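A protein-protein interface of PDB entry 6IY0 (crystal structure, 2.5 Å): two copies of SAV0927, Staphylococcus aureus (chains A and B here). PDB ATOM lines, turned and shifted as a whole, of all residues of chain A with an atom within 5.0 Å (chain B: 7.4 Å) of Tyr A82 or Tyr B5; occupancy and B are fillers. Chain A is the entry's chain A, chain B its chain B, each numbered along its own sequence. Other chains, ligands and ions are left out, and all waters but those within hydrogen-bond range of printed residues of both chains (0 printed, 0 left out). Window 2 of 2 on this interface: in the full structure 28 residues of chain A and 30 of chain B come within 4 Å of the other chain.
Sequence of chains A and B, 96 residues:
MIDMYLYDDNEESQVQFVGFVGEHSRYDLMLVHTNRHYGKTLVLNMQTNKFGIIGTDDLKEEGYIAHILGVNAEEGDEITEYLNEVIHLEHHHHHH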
ATOM      1  N   GLN A  16     -19.031 -20.265  14.794  1.00  0.00           N
ATOM      2  CA  GLN A  16     -18.715 -19.464  15.973  1.00  0.00           C
ATOM      3  C   GLN A  16     -18.619 -20.383  17.186  1.00  0.00           C
ATOM      4  O   GLN A  16     -19.625 -20.955  17.620  1.00  0.00           O
ATOM      5  CB  GLN A  16     -19.763 -18.373  16.189  1.00  0.00           C
ATOM      6  CG  GLN A  16     -19.580 -17.589  17.474  1.00  0.00           C
ATOM      7  CD  GLN A  16     -20.522 -16.405  17.579  1.00  0.00           C
ATOM      8  OE1 GLN A  16     -20.639 -15.779  18.634  1.00  0.00           O
ATOM      9  NE2 GLN A  16     -21.196 -16.087  16.480  1.00  0.00           N
ATOM     10  N   VAL A  18     -18.175 -20.569  21.083  1.00  0.00           N
ATOM     11  CA  VAL A  18     -18.386 -19.685  22.220  1.00  0.00           C
ATOM     12  C   VAL A  18     -18.357 -20.487  23.511  1.00  0.00           C
ATOM     13  O   VAL A  18     -18.742 -21.660  23.553  1.00  0.00           O
ATOM     14  CB  VAL A  18     -19.712 -18.900  22.106  1.00  0.00           C
ATOM     15  CG1 VAL A  18     -19.596 -17.838  21.031  1.00  0.00           C
ATOM     16  CG2 VAL A  18     -20.865 -19.840  21.810  1.00  0.00           C
ATOM     17  N   GLY A  19     -17.894 -19.835  24.571  1.00  0.00           N
ATOM     18  CA  GLY A  19     -17.890 -20.416  25.895  1.00  0.00           C
ATOM     19  C   GLY A  19     -18.150 -19.366  26.952  1.00  0.00           C
ATOM     20  O   GLY A  19     -17.525 -18.300  26.945  1.00  0.00           O
ATOM     21  N   PHE A  20     -19.077 -19.648  27.863  1.00  0.00           N
ATOM     22  CA  PHE A  20     -19.438 -18.695  28.901  1.00  0.00           C
ATOM     23  C   PHE A  20     -19.823 -19.454  30.161  1.00  0.00           C
ATOM     24  O   PHE A  20     -20.275 -20.600  30.101  1.00  0.00           O
ATOM     25  CB  PHE A  20     -20.587 -17.783  28.452  1.00  0.00           C
ATOM     26  CG  PHE A  20     -21.854 -18.518  28.117  1.00  0.00           C
ATOM     27  CD1 PHE A  20     -22.028 -19.101  26.872  1.00  0.00           C
ATOM     28  CD2 PHE A  20     -22.876 -18.619  29.047  1.00  0.00           C
ATOM     29  CE1 PHE A  20     -23.194 -19.778  26.563  1.00  0.00           C
ATOM     30  CE2 PHE A  20     -24.046 -19.293  28.742  1.00  0.00           C
ATOM     31  CZ  PHE A  20     -24.204 -19.874  27.500  1.00  0.00           C
ATOM     32  N   ASP A  77     -32.218 -21.723  30.452  1.00  0.00           N
ATOM     33  CA  ASP A  77     -32.469 -20.286  30.461  1.00  0.00           C
ATOM     34  C   ASP A  77     -31.170 -19.504  30.316  1.00  0.00           C
ATOM     35  O   ASP A  77     -31.136 -18.462  29.650  1.00  0.00           O
ATOM     36  CB  ASP A  77     -33.197 -19.884  31.744  1.00  0.00           C
ATOM     37  CG  ASP A  77     -34.565 -20.525  31.866  1.00  0.00           C
ATOM     38  OD1 ASP A  77     -34.919 -21.344  30.992  1.00  0.00           O
ATOM     39  OD2 ASP A  77     -35.285 -20.213  32.838  1.00  0.00           O
ATOM     40  N   GLU A  78     -30.089 -19.991  30.932  1.00  0.00           N
ATOM     41  CA  GLU A  78     -28.796 -19.330  30.790  1.00  0.00           C
ATOM     42  C   GLU A  78     -28.278 -19.443  29.362  1.00  0.00           C
ATOM     43  O   GLU A  78     -27.636 -18.516  28.854  1.00  0.00           O
ATOM     44  CB  GLU A  78     -27.794 -19.921  31.781  1.00  0.00           C
ATOM     45  CG  GLU A  78     -27.962 -19.406  33.204  1.00  0.00           C
ATOM     46  CD  GLU A  78     -26.901 -19.935  34.152  1.00  0.00           C
ATOM     47  OE1 GLU A  78     -26.138 -20.840  33.753  1.00  0.00           O
ATOM     48  OE2 GLU A  78     -26.830 -19.447  35.299  1.00  0.00           O
ATOM     49  N   ILE A  79     -28.546 -20.568  28.697  1.00  0.00           N
ATOM     50  CA  ILE A  79     -28.233 -20.676  27.277  1.00  0.00           C
ATOM     51  C   ILE A  79     -29.152 -19.771  26.467  1.00  0.00           C
ATOM     52  O   ILE A  79     -28.725 -19.138  25.494  1.00  0.00           O
ATOM     53  CB  ILE A  79     -28.325 -22.143  26.818  1.00  0.00           C
ATOM     54  CG1 ILE A  79     -27.306 -23.001  27.573  1.00  0.00           C
ATOM     55  CG2 ILE A  79     -28.104 -22.253  25.317  1.00  0.00           C
ATOM     56  CD1 ILE A  79     -27.366 -24.475  27.225  1.00  0.00           C
ATOM     57  N   THR A  80     -30.424 -19.685  26.864  1.00  0.00           N
ATOM     58  CA  THR A  80     -31.364 -18.804  26.177  1.00  0.00           C
ATOM     59  C   THR A  80     -30.977 -17.340  26.352  1.00  0.00           C
ATOM     60  O   THR A  80     -31.075 -16.549  25.406  1.00  0.00           O
ATOM     61  CB  THR A  80     -32.783 -19.053  26.693  1.00  0.00           C
ATOM     62  OG1 THR A  80     -33.218 -20.357  26.285  1.00  0.00           O
ATOM     63  CG2 THR A  80     -33.751 -18.011  26.148  1.00  0.00           C
ATOM     64  N   GLU A  81     -30.529 -16.963  27.552  1.00  0.00           N
ATOM     65  CA  GLU A  81     -30.097 -15.587  27.777  1.00  0.00           C
ATOM     66  C   GLU A  81     -28.890 -15.245  26.912  1.00  0.00           C
ATOM     67  O   GLU A  81     -28.772 -14.120  26.411  1.00  0.00           O
ATOM     68  CB  GLU A  81     -29.783 -15.372  29.258  1.00  0.00           C
ATOM     69  CG  GLU A  81     -28.942 -14.139  29.549  1.00  0.00           C
ATOM     70  CD  GLU A  81     -28.000 -14.342  30.719  1.00  0.00           C
ATOM     71  OE1 GLU A  81     -27.050 -15.144  30.587  1.00  0.00           O
ATOM     72  OE2 GLU A  81     -28.209 -13.701  31.770  1.00  0.00           O
ATOM     73  N   TYR A  82     -27.987 -16.207  26.710  1.00  0.00           N
ATOM     74  CA  TYR A  82     -26.861 -15.975  25.813  1.00  0.00           C
ATOM     75  C   TYR A  82     -27.302 -15.961  24.355  1.00  0.00           C
ATOM     76  O   TYR A  82     -26.751 -15.203  23.550  1.00  0.00           O
ATOM     77  CB  TYR A  82     -25.783 -17.039  26.030  1.00  0.00           C
ATOM     78  CG  TYR A  82     -24.506 -16.774  25.265  1.00  0.00           C
ATOM     79  CD1 TYR A  82     -23.456 -16.083  25.852  1.00  0.00           C
ATOM     80  CD2 TYR A  82     -24.352 -17.210  23.953  1.00  0.00           C
ATOM     81  CE1 TYR A  82     -22.287 -15.833  25.156  1.00  0.00           C
ATOM     82  CE2 TYR A  82     -23.188 -16.963  23.249  1.00  0.00           C
ATOM     83  CZ  TYR A  82     -22.158 -16.274  23.857  1.00  0.00           C
ATOM     84  OH  TYR A  82     -20.995 -16.023  23.170  1.00  0.00           O
ATOM     85  N   LEU A  83     -28.295 -16.779  24.000  1.00  0.00           N
ATOM     86  CA  LEU A  83     -28.660 -16.942  22.597  1.00  0.00           C
ATOM     87  C   LEU A  83     -29.459 -15.754  22.069  1.00  0.00           C
ATOM     88  O   LEU A  83     -29.209 -15.291  20.951  1.00  0.00           O
ATOM     89  CB  LEU A  83     -29.446 -18.240  22.409  1.00  0.00           C
ATOM     90  CG  LEU A  83     -28.605 -19.515  22.310  1.00  0.00           C
ATOM     91  CD1 LEU A  83     -29.481 -20.716  21.980  1.00  0.00           C
ATOM     92  CD2 LEU A  83     -27.492 -19.358  21.285  1.00  0.00           C
ATOM     93  N   ASN A  84     -30.426 -15.250  22.843  1.00  0.00           N
ATOM     94  CA  ASN A  84     -31.196 -14.103  22.371  1.00  0.00           C
ATOM     95  C   ASN A  84     -30.329 -12.857  22.254  1.00  0.00           C
ATOM     96  O   ASN A  84     -30.606 -11.984  21.425  1.00  0.00           O
ATOM     97  CB  ASN A  84     -32.401 -13.844  23.283  1.00  0.00           C
ATOM     98  CG  ASN A  84     -32.011 -13.517  24.720  1.00  0.00           C
ATOM     99  OD1 ASN A  84     -30.896 -13.080  25.002  1.00  0.00           O
ATOM    100  ND2 ASN A  84     -32.949 -13.720  25.638  1.00  0.00           N
ATOM    101  N   GLU A  85     -29.283 -12.759  23.080  1.00  0.00           N
ATOM    102  CA  GLU A  85     -28.330 -11.659  22.973  1.00  0.00           C
ATOM    103  C   GLU A  85     -27.675 -11.622  21.600  1.00  0.00           C
ATOM    104  O   GLU A  85     -27.510 -10.548  21.009  1.00  0.00           O
ATOM    105  CB  GLU A  85     -27.263 -11.792  24.060  1.00  0.00           C
ATOM    106  CG  GLU A  85     -26.327 -10.602  24.176  1.00  0.00           C
ATOM    107  CD  GLU A  85     -26.896  -9.492  25.035  1.00  0.00           C
ATOM    108  OE1 GLU A  85     -26.837  -8.319  24.608  1.00  0.00           O
ATOM    109  OE2 GLU A  85     -27.402  -9.793  26.137  1.00  0.00           O
ATOM    110  N   VAL A  86     -27.296 -12.783  21.082  1.00  0.00           N
ATOM    111  CA  VAL A  86     -26.526 -12.867  19.850  1.00  0.00           C
ATOM    112  C   VAL A  86     -27.416 -13.268  18.677  1.00  0.00           C
ATOM    113  O   VAL A  86     -27.963 -14.371  18.647  1.00  0.00           O
ATOM    114  CB  VAL A  86     -25.355 -13.852  20.012  1.00  0.00           C
ATOM    115  CG1 VAL A  86     -24.283 -13.586  18.968  1.00  0.00           C
ATOM    116  CG2 VAL A  86     -24.777 -13.752  21.417  1.00  0.00           C
ATOM    117  N   ILE B   2     -22.858 -15.894  34.671  1.00  0.00           N
ATOM    118  CA  ILE B   2     -22.643 -14.878  33.649  1.00  0.00           C
ATOM    119  C   ILE B   2     -21.573 -13.904  34.140  1.00  0.00           C
ATOM    120  O   ILE B   2     -21.550 -12.731  33.767  1.00  0.00           O
ATOM    121  CB  ILE B   2     -23.961 -14.156  33.292  1.00  0.00           C
ATOM    122  CG1 ILE B   2     -25.121 -15.155  33.234  1.00  0.00           C
ATOM    123  CG2 ILE B   2     -23.847 -13.456  31.946  1.00  0.00           C
ATOM    124  CD1 ILE B   2     -25.984 -15.179  34.479  1.00  0.00           C
ATOM    125  N   ASP B   3     -20.676 -14.410  34.990  1.00  0.00           N
ATOM    126  CA  ASP B   3     -19.580 -13.582  35.478  1.00  0.00           C
ATOM    127  C   ASP B   3     -18.519 -13.384  34.404  1.00  0.00           C
ATOM    128  O   ASP B   3     -18.013 -12.270  34.221  1.00  0.00           O
ATOM    129  CB  ASP B   3     -18.969 -14.206  36.735  1.00  0.00           C
ATOM    130  CG  ASP B   3     -17.715 -13.482  37.203  1.00  0.00           C
ATOM    131  OD1 ASP B   3     -16.632 -13.716  36.623  1.00  0.00           O
ATOM    132  OD2 ASP B   3     -17.811 -12.681  38.155  1.00  0.00           O
ATOM    133  N   MET B   4     -18.172 -14.444  33.681  1.00  0.00           N
ATOM    134  CA  MET B   4     -17.060 -14.381  32.741  1.00  0.00           C
ATOM    135  C   MET B   4     -17.401 -14.945  31.366  1.00  0.00           C
ATOM    136  O   MET B   4     -17.981 -16.025  31.248  1.00  0.00           O
ATOM    137  CB  MET B   4     -15.852 -15.123  33.321  1.00  0.00           C
ATOM    138  CG  MET B   4     -14.733 -15.376  32.326  1.00  0.00           C
ATOM    139  SD  MET B   4     -13.937 -13.730  31.650  1.00  0.00           S
ATOM    140  CE  MET B   4     -12.376 -13.648  32.815  1.00  0.00           C
ATOM    141  N   TYR B   5     -17.037 -14.196  30.327  1.00  0.00           N
ATOM    142  CA  TYR B   5     -17.128 -14.660  28.947  1.00  0.00           C
ATOM    143  C   TYR B   5     -15.792 -15.299  28.581  1.00  0.00           C
ATOM    144  O   TYR B   5     -14.786 -14.600  28.418  1.00  0.00           O
ATOM    145  CB  TYR B   5     -17.466 -13.503  28.009  1.00  0.00           C
ATOM    146  CG  TYR B   5     -18.949 -13.309  27.769  1.00  0.00           C
ATOM    147  CD1 TYR B   5     -19.414 -12.794  26.564  1.00  0.00           C
ATOM    148  CD2 TYR B   5     -19.882 -13.637  28.744  1.00  0.00           C
ATOM    149  CE1 TYR B   5     -20.767 -12.612  26.338  1.00  0.00           C
ATOM    150  CE2 TYR B   5     -21.237 -13.458  28.527  1.00  0.00           C
ATOM    151  CZ  TYR B   5     -21.674 -12.945  27.323  1.00  0.00           C
ATOM    152  OH  TYR B   5     -23.021 -12.767  27.103  1.00  0.00           O
ATOM    153  N   LEU B   6     -15.783 -16.628  28.455  1.00  0.00           N
ATOM    154  CA  LEU B   6     -14.523 -17.349  28.306  1.00  0.00           C
ATOM    155  C   LEU B   6     -13.862 -17.053  26.965  1.00  0.00           C
ATOM    156  O   LEU B   6     -12.683 -16.683  26.913  1.00  0.00           O
ATOM    157  CB  LEU B   6     -14.759 -18.850  28.473  1.00  0.00           C
ATOM    158  CG  LEU B   6     -15.468 -19.269  29.762  1.00  0.00           C
ATOM    159  CD1 LEU B   6     -15.641 -20.777  29.816  1.00  0.00           C
ATOM    160  CD2 LEU B   6     -14.699 -18.767  30.973  1.00  0.00           C
ATOM    161  N   TYR B   7     -14.601 -17.207  25.868  1.00  0.00           N
ATOM    162  CA  TYR B   7     -14.022 -17.019  24.545  1.00  0.00           C
ATOM    163  C   TYR B   7     -15.135 -16.835  23.525  1.00  0.00           C
ATOM    164  O   TYR B   7     -16.297 -17.171  23.774  1.00  0.00           O
ATOM    165  CB  TYR B   7     -13.122 -18.195  24.150  1.00  0.00           C
ATOM    166  CG  TYR B   7     -13.815 -19.541  24.163  1.00  0.00           C
ATOM    167  CD1 TYR B   7     -14.280 -20.117  22.988  1.00  0.00           C
ATOM    168  CD2 TYR B   7     -14.000 -20.238  25.349  1.00  0.00           C
ATOM    169  CE1 TYR B   7     -14.914 -21.347  22.996  1.00  0.00           C
ATOM    170  CE2 TYR B   7     -14.628 -21.468  25.368  1.00  0.00           C
ATOM    171  CZ  TYR B   7     -15.086 -22.017  24.191  1.00  0.00           C
ATOM    172  OH  TYR B   7     -15.714 -23.242  24.210  1.00  0.00           O
ATOM    173  N   ASP B   8     -14.753 -16.297  22.364  1.00  0.00           N
ATOM    174  CA  ASP B   8     -15.692 -16.057  21.269  1.00  0.00           C
ATOM    175  C   ASP B   8     -14.861 -15.886  19.996  1.00  0.00           C
ATOM    176  O   ASP B   8     -14.340 -14.798  19.742  1.00  0.00           O
ATOM    177  CB  ASP B   8     -16.558 -14.833  21.535  1.00  0.00           C
ATOM    178  CG  ASP B   8     -17.801 -14.797  20.665  1.00  0.00           C
ATOM    179  OD1 ASP B   8     -18.918 -14.662  21.211  1.00  0.00           O
ATOM    180  OD2 ASP B   8     -17.662 -14.915  19.430  1.00  0.00           O
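No position is printed for both chains.
Of the 7 printed residues of chain B, 6 touch a printed residue of chain A.
Printed residues of chain B that touch a printed residue of chain A: Ile B2, Met B4, Tyr B5, Leu B6, Tyr B7 and Asp B8.
Hydrophobic or aromatic side chains of chain A that line the printed part of chain B: Val A18 and Tyr A82.
Of chain B, only Tyr B5 (3.6 Å) and Asp B8 (3.2 Å) come within 4 Å of Tyr A82.
Of chain A, only Gly A19 and Tyr A82 come within 4 Å of Tyr B5.
Of the printed residues of chain A, Ile B2 touches Glu A81.
Of the printed residues of chain A, Leu B6 touches Gly A19.
Of the printed residues of chain A, Met B4 touches Phe A20 (3.8 Å).
Printed residues of chain A within 4 Å of Asp B8: Gln A16 (3.2 Å), Val A18 (3.3 Å) and Tyr A82 (3.2 Å).
Printed residues of chain A within 4 Å of Tyr B7: Val A18 and Gly A19.
Asn A84 touches none of the printed residues of chain B.
Glu A78 touches none of the printed residues of chain B.
The nearest printed residue of chain B that does not touch Gly A19 is Met B4 (4.9 Å).
The side-chain amide oxygen of Asn A84 lies close to the backbone carbonyl oxygen of Glu A81, at 2.8 Å.
Among the printed residues, merely in contact across the chains: Val A18 with Asp B8, Gly A19 with Tyr B5, Phe A20 with Met B4, Glu A81 with Ile B2 and Tyr A82 with Tyr B5.
OH of Tyr A82 sits at hydrogen-bond distance from OD1 of Asp B8 (3.2 Å).
The backbone carbonyl oxygen (O) of Gly A19 lies within hydrogen-bond range of the backbone NH (N) of Leu B6 (2.8 Å).
The backbone NH of Gly A19 sits at hydrogen-bond distance from the backbone carbonyl oxygen of Tyr B7 (3.2 Å).
The side-chain hydroxyl (OH) of Tyr B7 is in hydrogen-bond range of the backbone carbonyl oxygen (O) of Val A18 (3.5 Å).
OE1 of Gln A16 sits close to OD2 of Asp B8 (3.2 Å).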
